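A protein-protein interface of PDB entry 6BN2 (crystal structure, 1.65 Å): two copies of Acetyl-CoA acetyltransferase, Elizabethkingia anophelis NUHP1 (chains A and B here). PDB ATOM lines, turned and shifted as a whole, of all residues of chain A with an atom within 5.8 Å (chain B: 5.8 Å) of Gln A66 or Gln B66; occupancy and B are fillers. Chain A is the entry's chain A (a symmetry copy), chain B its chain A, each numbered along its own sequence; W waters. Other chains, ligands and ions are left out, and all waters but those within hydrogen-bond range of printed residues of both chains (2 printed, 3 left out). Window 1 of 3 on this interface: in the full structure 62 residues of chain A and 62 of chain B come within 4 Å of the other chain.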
ATOM      1  N   ASN A  63      -3.393  15.850  26.649  1.00  0.00           N
ATOM      2  CA  ASN A  63      -3.314  16.290  25.256  1.00  0.00           C
ATOM      3  C   ASN A  63      -4.659  15.977  24.609  1.00  0.00           C
ATOM      4  O   ASN A  63      -4.981  14.806  24.435  1.00  0.00           O
ATOM      5  CB  ASN A  63      -2.148  15.551  24.594  1.00  0.00           C
ATOM      6  CG  ASN A  63      -1.801  16.051  23.197  1.00  0.00           C
ATOM      7  OD1 ASN A  63      -2.203  17.135  22.729  1.00  0.00           O
ATOM      8  ND2 ASN A  63      -1.024  15.254  22.528  1.00  0.00           N
ATOM      9  N   VAL A  64      -5.474  16.997  24.322  1.00  0.00           N
ATOM     10  CA  VAL A  64      -6.854  16.737  23.919  1.00  0.00           C
ATOM     11  C   VAL A  64      -6.948  16.473  22.423  1.00  0.00           C
ATOM     12  O   VAL A  64      -7.775  15.659  21.974  1.00  0.00           O
ATOM     13  CB  VAL A  64      -7.748  17.916  24.318  1.00  0.00           C
ATOM     14  CG1 VAL A  64      -9.186  17.670  23.839  1.00  0.00           C
ATOM     15  CG2 VAL A  64      -7.704  18.084  25.835  1.00  0.00           C
ATOM     16  N   LEU A  65      -6.124  17.158  21.630  1.00  0.00           N
ATOM     17  CA  LEU A  65      -6.275  17.199  20.173  1.00  0.00           C
ATOM     18  C   LEU A  65      -4.994  16.636  19.568  1.00  0.00           C
ATOM     19  O   LEU A  65      -4.056  17.366  19.231  1.00  0.00           O
ATOM     20  CB  LEU A  65      -6.584  18.658  19.708  1.00  0.00           C
ATOM     21  CG  LEU A  65      -7.878  19.159  20.357  1.00  0.00           C
ATOM     22  CD1 LEU A  65      -8.019  20.663  20.211  1.00  0.00           C
ATOM     23  CD2 LEU A  65      -9.115  18.442  19.780  1.00  0.00           C
ATOM     24  N   GLN A  66      -4.946  15.308  19.475  1.00  0.00           N
ATOM     25  CA  GLN A  66      -3.720  14.591  19.135  1.00  0.00           C
ATOM     26  C   GLN A  66      -3.522  14.421  17.634  1.00  0.00           C
ATOM     27  O   GLN A  66      -2.464  13.938  17.219  1.00  0.00           O
ATOM     28  CB  GLN A  66      -3.737  13.218  19.814  1.00  0.00           C
ATOM     29  CG  GLN A  66      -3.801  13.362  21.353  1.00  0.00           C
ATOM     30  CD  GLN A  66      -4.067  12.070  22.102  1.00  0.00           C
ATOM     31  OE1 GLN A  66      -4.060  10.983  21.524  1.00  0.00           O
ATOM     32  NE2 GLN A  66      -4.304  12.186  23.415  1.00  0.00           N
ATOM     33  N   ALA A  67      -4.507  14.798  16.818  1.00  0.00           N
ATOM     34  CA  ALA A  67      -4.440  14.489  15.396  1.00  0.00           C
ATOM     35  C   ALA A  67      -3.250  15.170  14.744  1.00  0.00           C
ATOM     36  O   ALA A  67      -3.044  16.386  14.890  1.00  0.00           O
ATOM     37  CB  ALA A  67      -5.728  14.924  14.688  1.00  0.00           C
ATOM     38  N   GLY A  68      -2.486  14.380  13.985  1.00  0.00           N
ATOM     39  CA  GLY A  68      -1.374  14.889  13.222  1.00  0.00           C
ATOM     40  C   GLY A  68      -0.132  15.190  14.025  1.00  0.00           C
ATOM     41  O   GLY A  68       0.857  15.657  13.440  1.00  0.00           O
ATOM     42  N   GLU A  69      -0.147  14.942  15.341  1.00  0.00           N
ATOM     43  CA  GLU A  69       1.057  15.127  16.143  1.00  0.00           C
ATOM     44  C   GLU A  69       2.071  14.018  15.930  1.00  0.00           C
ATOM     45  O   GLU A  69       3.210  14.140  16.388  1.00  0.00           O
ATOM     46  CB  GLU A  69       0.703  15.194  17.626  1.00  0.00           C
ATOM     47  CG  GLU A  69      -0.199  16.361  17.963  1.00  0.00           C
ATOM     48  CD  GLU A  69      -0.504  16.397  19.444  1.00  0.00           C
ATOM     49  OE1 GLU A  69      -0.877  17.481  19.937  1.00  0.00           O
ATOM     50  OE2 GLU A  69      -0.383  15.319  20.103  1.00  0.00           O
ATOM     51  N   GLY A  70       1.692  12.949  15.239  1.00  0.00           N
ATOM     52  CA  GLY A  70       2.588  11.830  15.063  1.00  0.00           C
ATOM     53  C   GLY A  70       2.422  10.788  16.155  1.00  0.00           C
ATOM     54  O   GLY A  70       1.704  10.965  17.146  1.00  0.00           O
ATOM     55  N   PRO A  73       2.538  10.854  21.045  1.00  0.00           N
ATOM     56  CA  PRO A  73       2.863  12.246  21.406  1.00  0.00           C
ATOM     57  C   PRO A  73       3.554  12.379  22.756  1.00  0.00           C
ATOM     58  O   PRO A  73       4.446  13.225  22.891  1.00  0.00           O
ATOM     59  CB  PRO A  73       1.500  12.956  21.390  1.00  0.00           C
ATOM     60  CG  PRO A  73       0.473  11.924  21.077  1.00  0.00           C
ATOM     61  CD  PRO A  73       1.140  10.668  20.629  1.00  0.00           C
ATOM     62  N   ALA A  91      -0.168   9.429  26.936  1.00  0.00           N
ATOM     63  CA  ALA A  91      -0.950  10.654  26.769  1.00  0.00           C
ATOM     64  C   ALA A  91      -2.372  10.430  27.267  1.00  0.00           C
ATOM     65  O   ALA A  91      -2.966   9.375  27.019  1.00  0.00           O
ATOM     66  CB  ALA A  91      -0.973  11.108  25.300  1.00  0.00           C
ATOM     67  N   VAL A  92      -2.923  11.419  27.974  1.00  0.00           N
ATOM     68  CA  VAL A  92      -4.246  11.258  28.582  1.00  0.00           C
ATOM     69  C   VAL A  92      -5.189  12.347  28.083  1.00  0.00           C
ATOM     70  O   VAL A  92      -4.781  13.488  27.821  1.00  0.00           O
ATOM     71  CB  VAL A  92      -4.159  11.210  30.128  1.00  0.00           C
ATOM     72  CG1 VAL A  92      -2.715  11.120  30.598  1.00  0.00           C
ATOM     73  CG2 VAL A  92      -4.892  12.334  30.792  1.00  0.00           C
ATOM     74  N   ASN A  93      -6.450  11.973  27.891  1.00  0.00           N
ATOM     75  CA  ASN A  93      -7.460  12.866  27.323  1.00  0.00           C
ATOM     76  C   ASN A  93      -8.738  12.785  28.157  1.00  0.00           C
ATOM     77  O   ASN A  93      -9.554  11.869  27.993  1.00  0.00           O
ATOM     78  CB  ASN A  93      -7.720  12.504  25.864  1.00  0.00           C
ATOM     79  CG  ASN A  93      -8.780  13.382  25.223  1.00  0.00           C
ATOM     80  OD1 ASN A  93      -9.275  14.346  25.816  1.00  0.00           O
ATOM     81  ND2 ASN A  93      -9.143  13.041  23.991  1.00  0.00           N
ATOM     82  N   GLU A 124      -0.690  21.432  24.431  1.00  0.00           N
ATOM     83  CA  GLU A 124      -1.658  21.615  23.361  1.00  0.00           C
ATOM     84  C   GLU A 124      -1.124  22.669  22.410  1.00  0.00           C
ATOM     85  O   GLU A 124      -0.618  23.707  22.842  1.00  0.00           O
ATOM     86  CB  GLU A 124      -3.031  22.051  23.895  1.00  0.00           C
ATOM     87  CG  GLU A 124      -4.184  21.595  22.988  1.00  0.00           C
ATOM     88  CD  GLU A 124      -4.514  20.114  23.196  1.00  0.00           C
ATOM     89  OE1 GLU A 124      -4.937  19.747  24.322  1.00  0.00           O
ATOM     90  OE2 GLU A 124      -4.320  19.324  22.252  1.00  0.00           O
ATOM     91  N   TYR A 132     -10.283  17.560   9.015  1.00  0.00           N
ATOM     92  CA  TYR A 132     -10.427  16.127   8.761  1.00  0.00           C
ATOM     93  C   TYR A 132     -11.245  15.877   7.507  1.00  0.00           C
ATOM     94  O   TYR A 132     -12.271  16.525   7.289  1.00  0.00           O
ATOM     95  CB  TYR A 132     -11.170  15.446   9.916  1.00  0.00           C
ATOM     96  CG  TYR A 132     -10.622  15.657  11.300  1.00  0.00           C
ATOM     97  CD1 TYR A 132      -9.254  15.815  11.529  1.00  0.00           C
ATOM     98  CD2 TYR A 132     -11.487  15.682  12.392  1.00  0.00           C
ATOM     99  CE1 TYR A 132      -8.771  16.009  12.837  1.00  0.00           C
ATOM    100  CE2 TYR A 132     -11.021  15.854  13.677  1.00  0.00           C
ATOM    101  CZ  TYR A 132      -9.665  16.009  13.898  1.00  0.00           C
ATOM    102  OH  TYR A 132      -9.230  16.184  15.197  1.00  0.00           O
ATOM    103  N   ASP A 153     -13.612  17.926  17.702  1.00  0.00           N
ATOM    104  CA  ASP A 153     -13.159  17.132  18.837  1.00  0.00           C
ATOM    105  C   ASP A 153     -12.981  17.963  20.100  1.00  0.00           C
ATOM    106  O   ASP A 153     -13.018  17.414  21.208  1.00  0.00           O
ATOM    107  CB  ASP A 153     -11.834  16.427  18.499  1.00  0.00           C
ATOM    108  CG  ASP A 153     -11.979  15.369  17.397  1.00  0.00           C
ATOM    109  OD1 ASP A 153     -13.112  14.892  17.138  1.00  0.00           O
ATOM    110  OD2 ASP A 153     -10.939  14.996  16.801  1.00  0.00           O
ATOM    111  N   ASN B  63      -7.314   4.308  23.331  1.00  0.00           N
ATOM    112  CA  ASN B  63      -7.817   4.783  22.042  1.00  0.00           C
ATOM    113  C   ASN B  63      -6.680   5.546  21.370  1.00  0.00           C
ATOM    114  O   ASN B  63      -6.309   6.613  21.850  1.00  0.00           O
ATOM    115  CB  ASN B  63      -9.045   5.657  22.307  1.00  0.00           C
ATOM    116  CG  ASN B  63      -9.810   6.062  21.053  1.00  0.00           C
ATOM    117  OD1 ASN B  63      -9.657   5.516  19.942  1.00  0.00           O
ATOM    118  ND2 ASN B  63     -10.663   7.023  21.241  1.00  0.00           N
ATOM    119  N   VAL B  64      -6.076   4.983  20.319  1.00  0.00           N
ATOM    120  CA  VAL B  64      -4.843   5.560  19.790  1.00  0.00           C
ATOM    121  C   VAL B  64      -5.141   6.674  18.796  1.00  0.00           C
ATOM    122  O   VAL B  64      -4.399   7.668  18.715  1.00  0.00           O
ATOM    123  CB  VAL B  64      -3.988   4.468  19.138  1.00  0.00           C
ATOM    124  CG1 VAL B  64      -2.723   5.085  18.527  1.00  0.00           C
ATOM    125  CG2 VAL B  64      -3.627   3.423  20.191  1.00  0.00           C
ATOM    126  N   LEU B  65      -6.214   6.524  18.018  1.00  0.00           N
ATOM    127  CA  LEU B  65      -6.476   7.377  16.855  1.00  0.00           C
ATOM    128  C   LEU B  65      -7.816   8.066  17.090  1.00  0.00           C
ATOM    129  O   LEU B  65      -8.875   7.598  16.660  1.00  0.00           O
ATOM    130  CB  LEU B  65      -6.447   6.522  15.548  1.00  0.00           C
ATOM    131  CG  LEU B  65      -5.077   5.858  15.378  1.00  0.00           C
ATOM    132  CD1 LEU B  65      -5.124   4.761  14.330  1.00  0.00           C
ATOM    133  CD2 LEU B  65      -3.986   6.890  15.030  1.00  0.00           C
ATOM    134  N   GLN B  66      -7.762   9.175  17.827  1.00  0.00           N
ATOM    135  CA  GLN B  66      -8.961   9.833  18.339  1.00  0.00           C
ATOM    136  C   GLN B  66      -9.549  10.847  17.366  1.00  0.00           C
ATOM    137  O   GLN B  66     -10.630  11.379  17.634  1.00  0.00           O
ATOM    138  CB  GLN B  66      -8.628  10.522  19.666  1.00  0.00           C
ATOM    139  CG  GLN B  66      -8.154   9.493  20.721  1.00  0.00           C
ATOM    140  CD  GLN B  66      -7.571  10.099  21.983  1.00  0.00           C
ATOM    141  OE1 GLN B  66      -7.635  11.310  22.200  1.00  0.00           O
ATOM    142  NE2 GLN B  66      -6.992   9.245  22.836  1.00  0.00           N
ATOM    143  N   ALA B  67      -8.868  11.127  16.254  1.00  0.00           N
ATOM    144  CA  ALA B  67      -9.296  12.217  15.387  1.00  0.00           C
ATOM    145  C   ALA B  67     -10.679  11.952  14.819  1.00  0.00           C
ATOM    146  O   ALA B  67     -10.950  10.878  14.259  1.00  0.00           O
ATOM    147  CB  ALA B  67      -8.302  12.415  14.238  1.00  0.00           C
ATOM    148  N   GLY B  68     -11.544  12.963  14.931  1.00  0.00           N
ATOM    149  CA  GLY B  68     -12.868  12.909  14.360  1.00  0.00           C
ATOM    150  C   GLY B  68     -13.861  12.072  15.128  1.00  0.00           C
ATOM    151  O   GLY B  68     -15.013  11.957  14.681  1.00  0.00           O
ATOM    152  N   GLU B  69     -13.460  11.484  16.262  1.00  0.00           N
ATOM    153  CA  GLU B  69     -14.407  10.744  17.087  1.00  0.00           C
ATOM    154  C   GLU B  69     -15.331  11.659  17.871  1.00  0.00           C
ATOM    155  O   GLU B  69     -16.305  11.180  18.458  1.00  0.00           O
ATOM    156  CB  GLU B  69     -13.665   9.838  18.066  1.00  0.00           C
ATOM    157  CG  GLU B  69     -12.819   8.792  17.373  1.00  0.00           C
ATOM    158  CD  GLU B  69     -12.121   7.907  18.382  1.00  0.00           C
ATOM    159  OE1 GLU B  69     -11.731   6.785  18.002  1.00  0.00           O
ATOM    160  OE2 GLU B  69     -11.953   8.360  19.556  1.00  0.00           O
ATOM    161  N   GLY B  70     -15.059  12.959  17.885  1.00  0.00           N
ATOM    162  CA  GLY B  70     -15.859  13.870  18.669  1.00  0.00           C
ATOM    163  C   GLY B  70     -15.300  14.062  20.068  1.00  0.00           C
ATOM    164  O   GLY B  70     -14.356  13.397  20.510  1.00  0.00           O
ATOM    165  N   PRO B  73     -14.066  11.076  23.740  1.00  0.00           N
ATOM    166  CA  PRO B  73     -14.407   9.722  23.270  1.00  0.00           C
ATOM    167  C   PRO B  73     -14.707   8.744  24.397  1.00  0.00           C
ATOM    168  O   PRO B  73     -15.603   7.905  24.240  1.00  0.00           O
ATOM    169  CB  PRO B  73     -13.175   9.294  22.457  1.00  0.00           C
ATOM    170  CG  PRO B  73     -12.183  10.400  22.554  1.00  0.00           C
ATOM    171  CD  PRO B  73     -12.825  11.605  23.152  1.00  0.00           C
ATOM    172  N   ALA B  91      -9.714   8.945  28.277  1.00  0.00           N
ATOM    173  CA  ALA B  91      -9.128   8.143  27.203  1.00  0.00           C
ATOM    174  C   ALA B  91      -7.608   8.158  27.319  1.00  0.00           C
ATOM    175  O   ALA B  91      -7.010   9.202  27.598  1.00  0.00           O
ATOM    176  CB  ALA B  91      -9.555   8.662  25.820  1.00  0.00           C
ATOM    177  N   VAL B  92      -6.980   7.000  27.106  1.00  0.00           N
ATOM    178  CA  VAL B  92      -5.532   6.889  27.294  1.00  0.00           C
ATOM    179  C   VAL B  92      -4.870   6.409  26.007  1.00  0.00           C
ATOM    180  O   VAL B  92      -5.441   5.619  25.241  1.00  0.00           O
ATOM    181  CB  VAL B  92      -5.182   5.995  28.511  1.00  0.00           C
ATOM    182  CG1 VAL B  92      -6.425   5.650  29.318  1.00  0.00           C
ATOM    183  CG2 VAL B  92      -4.404   4.773  28.136  1.00  0.00           C
ATOM    184  N   ASN B  93      -3.682   6.941  25.738  1.00  0.00           N
ATOM    185  CA  ASN B  93      -2.957   6.664  24.498  1.00  0.00           C
ATOM    186  C   ASN B  93      -1.497   6.351  24.821  1.00  0.00           C
ATOM    187  O   ASN B  93      -0.675   7.256  25.019  1.00  0.00           O
ATOM    188  CB  ASN B  93      -3.078   7.850  23.544  1.00  0.00           C
ATOM    189  CG  ASN B  93      -2.324   7.634  22.243  1.00  0.00           C
ATOM    190  OD1 ASN B  93      -1.777   6.558  21.977  1.00  0.00           O
ATOM    191  ND2 ASN B  93      -2.285   8.676  21.420  1.00  0.00           N
ATOM    192  N   GLU B 124     -11.040   0.935  19.073  1.00  0.00           N
ATOM    193  CA  GLU B 124     -10.427   1.520  17.891  1.00  0.00           C
ATOM    194  C   GLU B 124     -11.300   1.200  16.693  1.00  0.00           C
ATOM    195  O   GLU B 124     -11.762   0.067  16.538  1.00  0.00           O
ATOM    196  CB  GLU B 124      -9.007   0.983  17.653  1.00  0.00           C
ATOM    197  CG  GLU B 124      -8.112   1.997  16.924  1.00  0.00           C
ATOM    198  CD  GLU B 124      -7.599   3.083  17.875  1.00  0.00           C
ATOM    199  OE1 GLU B 124      -6.849   2.742  18.824  1.00  0.00           O
ATOM    200  OE2 GLU B 124      -7.971   4.258  17.690  1.00  0.00           O
ATOM    201  N   TYR B 132      -5.763  14.137   7.134  1.00  0.00           N
ATOM    202  CA  TYR B 132      -5.559  15.443   7.760  1.00  0.00           C
ATOM    203  C   TYR B 132      -5.101  16.469   6.740  1.00  0.00           C
ATOM    204  O   TYR B 132      -4.240  16.180   5.905  1.00  0.00           O
ATOM    205  CB  TYR B 132      -4.466  15.365   8.831  1.00  0.00           C
ATOM    206  CG  TYR B 132      -4.627  14.318   9.897  1.00  0.00           C
ATOM    207  CD1 TYR B 132      -5.887  13.926  10.354  1.00  0.00           C
ATOM    208  CD2 TYR B 132      -3.500  13.727  10.465  1.00  0.00           C
ATOM    209  CE1 TYR B 132      -6.005  12.944  11.356  1.00  0.00           C
ATOM    210  CE2 TYR B 132      -3.607  12.778  11.458  1.00  0.00           C
ATOM    211  CZ  TYR B 132      -4.856  12.395  11.907  1.00  0.00           C
ATOM    212  OH  TYR B 132      -4.930  11.438  12.900  1.00  0.00           O
ATOM    213  N   ASP B 153      -0.211   8.967  12.532  1.00  0.00           N
ATOM    214  CA  ASP B 153      -0.256   8.878  13.985  1.00  0.00           C
ATOM    215  C   ASP B 153      -0.155   7.445  14.489  1.00  0.00           C
ATOM    216  O   ASP B 153       0.238   7.223  15.641  1.00  0.00           O
ATOM    217  CB  ASP B 153      -1.549   9.516  14.519  1.00  0.00           C
ATOM    218  CG  ASP B 153      -1.616  11.031  14.283  1.00  0.00           C
ATOM    219  OD1 ASP B 153      -0.559  11.673  14.059  1.00  0.00           O
ATOM    220  OD2 ASP B 153      -2.741  11.586  14.344  1.00  0.00           O
HETATM  221  O   HOH W   1      -5.109  10.154  19.103  1.00  0.00           O
HETATM  222  O   HOH W   2      -7.222  13.515  20.583  1.00  0.00           O
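Water W1 lies within hydrogen-bond range of O of Val B64 (2.6 Å), OE1 of Gln A66 (2.8 Å) and N of Gln B66 (3.1 Å).
Water W2 lies within hydrogen-bond range of O of Val A64, OE1 of Gln B66 and N of Gln A66.
Among the printed residues, pairs that only touch across the chains: Gln A66 with Gln B66, Gln A66 with Asp B153, Ala A67 with Ala B67, Ala A67 with Tyr B132, Ala A67 with Asp B153, Gly A68 with Tyr B132, Glu A69 with Asp B153, Ala A91 with Val B92, Val A92 with Ala B91, Tyr A132 with Ala B67, Tyr A132 with Gly B68, Asp A153 with Gln B66, Asp A153 with Ala B67 and Asp A153 with Glu B69.
The side-chain carboxylate (OD1) of Asp A153 sits at hydrogen-bond distance from the backbone NH (N) of Gly B70 (2.8 Å).
O of Ala B91 sits at hydrogen-bond distance from N of Asn A93 (2.8 Å).
N of Asn B93 lies within hydrogen-bond range of O of Ala A91, 2.8 Å away.
N of Gly A68 sits at hydrogen-bond distance from OD2 of Asp B153 (2.8 Å).
The side-chain carboxylate (OD1) of Asp B153 lies within hydrogen-bond range of the backbone NH (N) of Gly A70 (2.8 Å).
The side-chain amide nitrogen (ND2) of Asn A93 sits at hydrogen-bond distance from the side-chain amide oxygen (OE1) of Gln B66, 2.9 Å away.
The backbone NH (N) of Gly B68 lies within hydrogen-bond range of the side-chain carboxylate (OD2) of Asp A153, at 2.8 Å.
ND2 of Asn B93 is in hydrogen-bond range of OE1 of Gln A66 (2.9 Å).
Hydrophobic or aromatic side chains of chain A within 4 Å of the printed part of chain B: Ala A67, Ala A91 and Tyr A132.
Hydrophobic or aromatic side chains of chain B that line the printed part of chain A: Ala B67, Ala B91 and Tyr B132.
Among the printed residues, no Asp or Glu carboxylate lies within 4 Å of a Lys or Arg side-chain nitrogen of the other chain.
Gln A66 touches Asn B93, and with the chains exchanged Asn A93 touches Gln B66.
Ala A67 touches Tyr B132, and with the chains exchanged Tyr A132 touches Ala B67.
Ala A67 touches Asp B153, and with the chains exchanged Asp A153 touches Ala B67.
Ala A91 touches Val B92, and with the chains exchanged Val A92 touches Ala B91.
Positions printed for both chains: 63, 64, 65, 66, 67, 68, 69, 70, 73, 91, 92, 93, 124, 132 and 153.
Of the 22 pairs that touch across the chains among the printed residues, 22 have their exchanged pair printed and touching as well.
The side-chain carboxylate (OD2) of Asp B153 is in hydrogen-bond range of the side-chain hydroxyl (OH) of Tyr B132 (2.6 Å).
O of Asn A63 lies within hydrogen-bond range of NE2 of Gln A66 (2.9 Å).
NE2 of Gln B66 lies within hydrogen-bond range of O of Asn B63, at 2.9 Å.
The side-chain amide nitrogen of Asn B63 lies within hydrogen-bond range of the side-chain carboxylate of Glu B69.
The side-chain amide nitrogen (ND2) of Asn A63 sits at hydrogen-bond distance from the side-chain carboxylate (OE2) of Glu A69 (2.5 Å).
The backbone NH of Asn A63 sits at hydrogen-bond distance from the backbone carbonyl oxygen of Val A92.
Gln A66 touches three residues of chain B.
Gln B66 touches just these residues of chain A: Gln A66 (3.6 Å), Asn A93 (2.9 Å) and Asp A153 (3.7 Å).
Of the printed residues of chain A, Asp B153 touches Gln A66, Ala A67, Gly A68, Glu A69 and Gly A70.
Of the printed residues of chain B, Gly A70 touches Asp B153 (2.8 Å).
Of the printed residues of chain A, Asn B93 touches Gln A66 and Ala A91.
Printed residues of chain A within 4 Å of Glu B69: Asp A153.
Printed residues of chain B within 4 Å of Tyr A132: Ala B67 and Gly B68.
Leu B65 touches none of the printed residues of chain A.
The nearest residue of chain B that does not touch Gln A66 is Val B64 (4.4 Å).
The nearest residue of chain A that does not touch Gln B66 is Val A64 (4.4 Å).
The nearest printed residue of chain A that does not touch Gly B70 is Asn A93 (6.3 Å).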
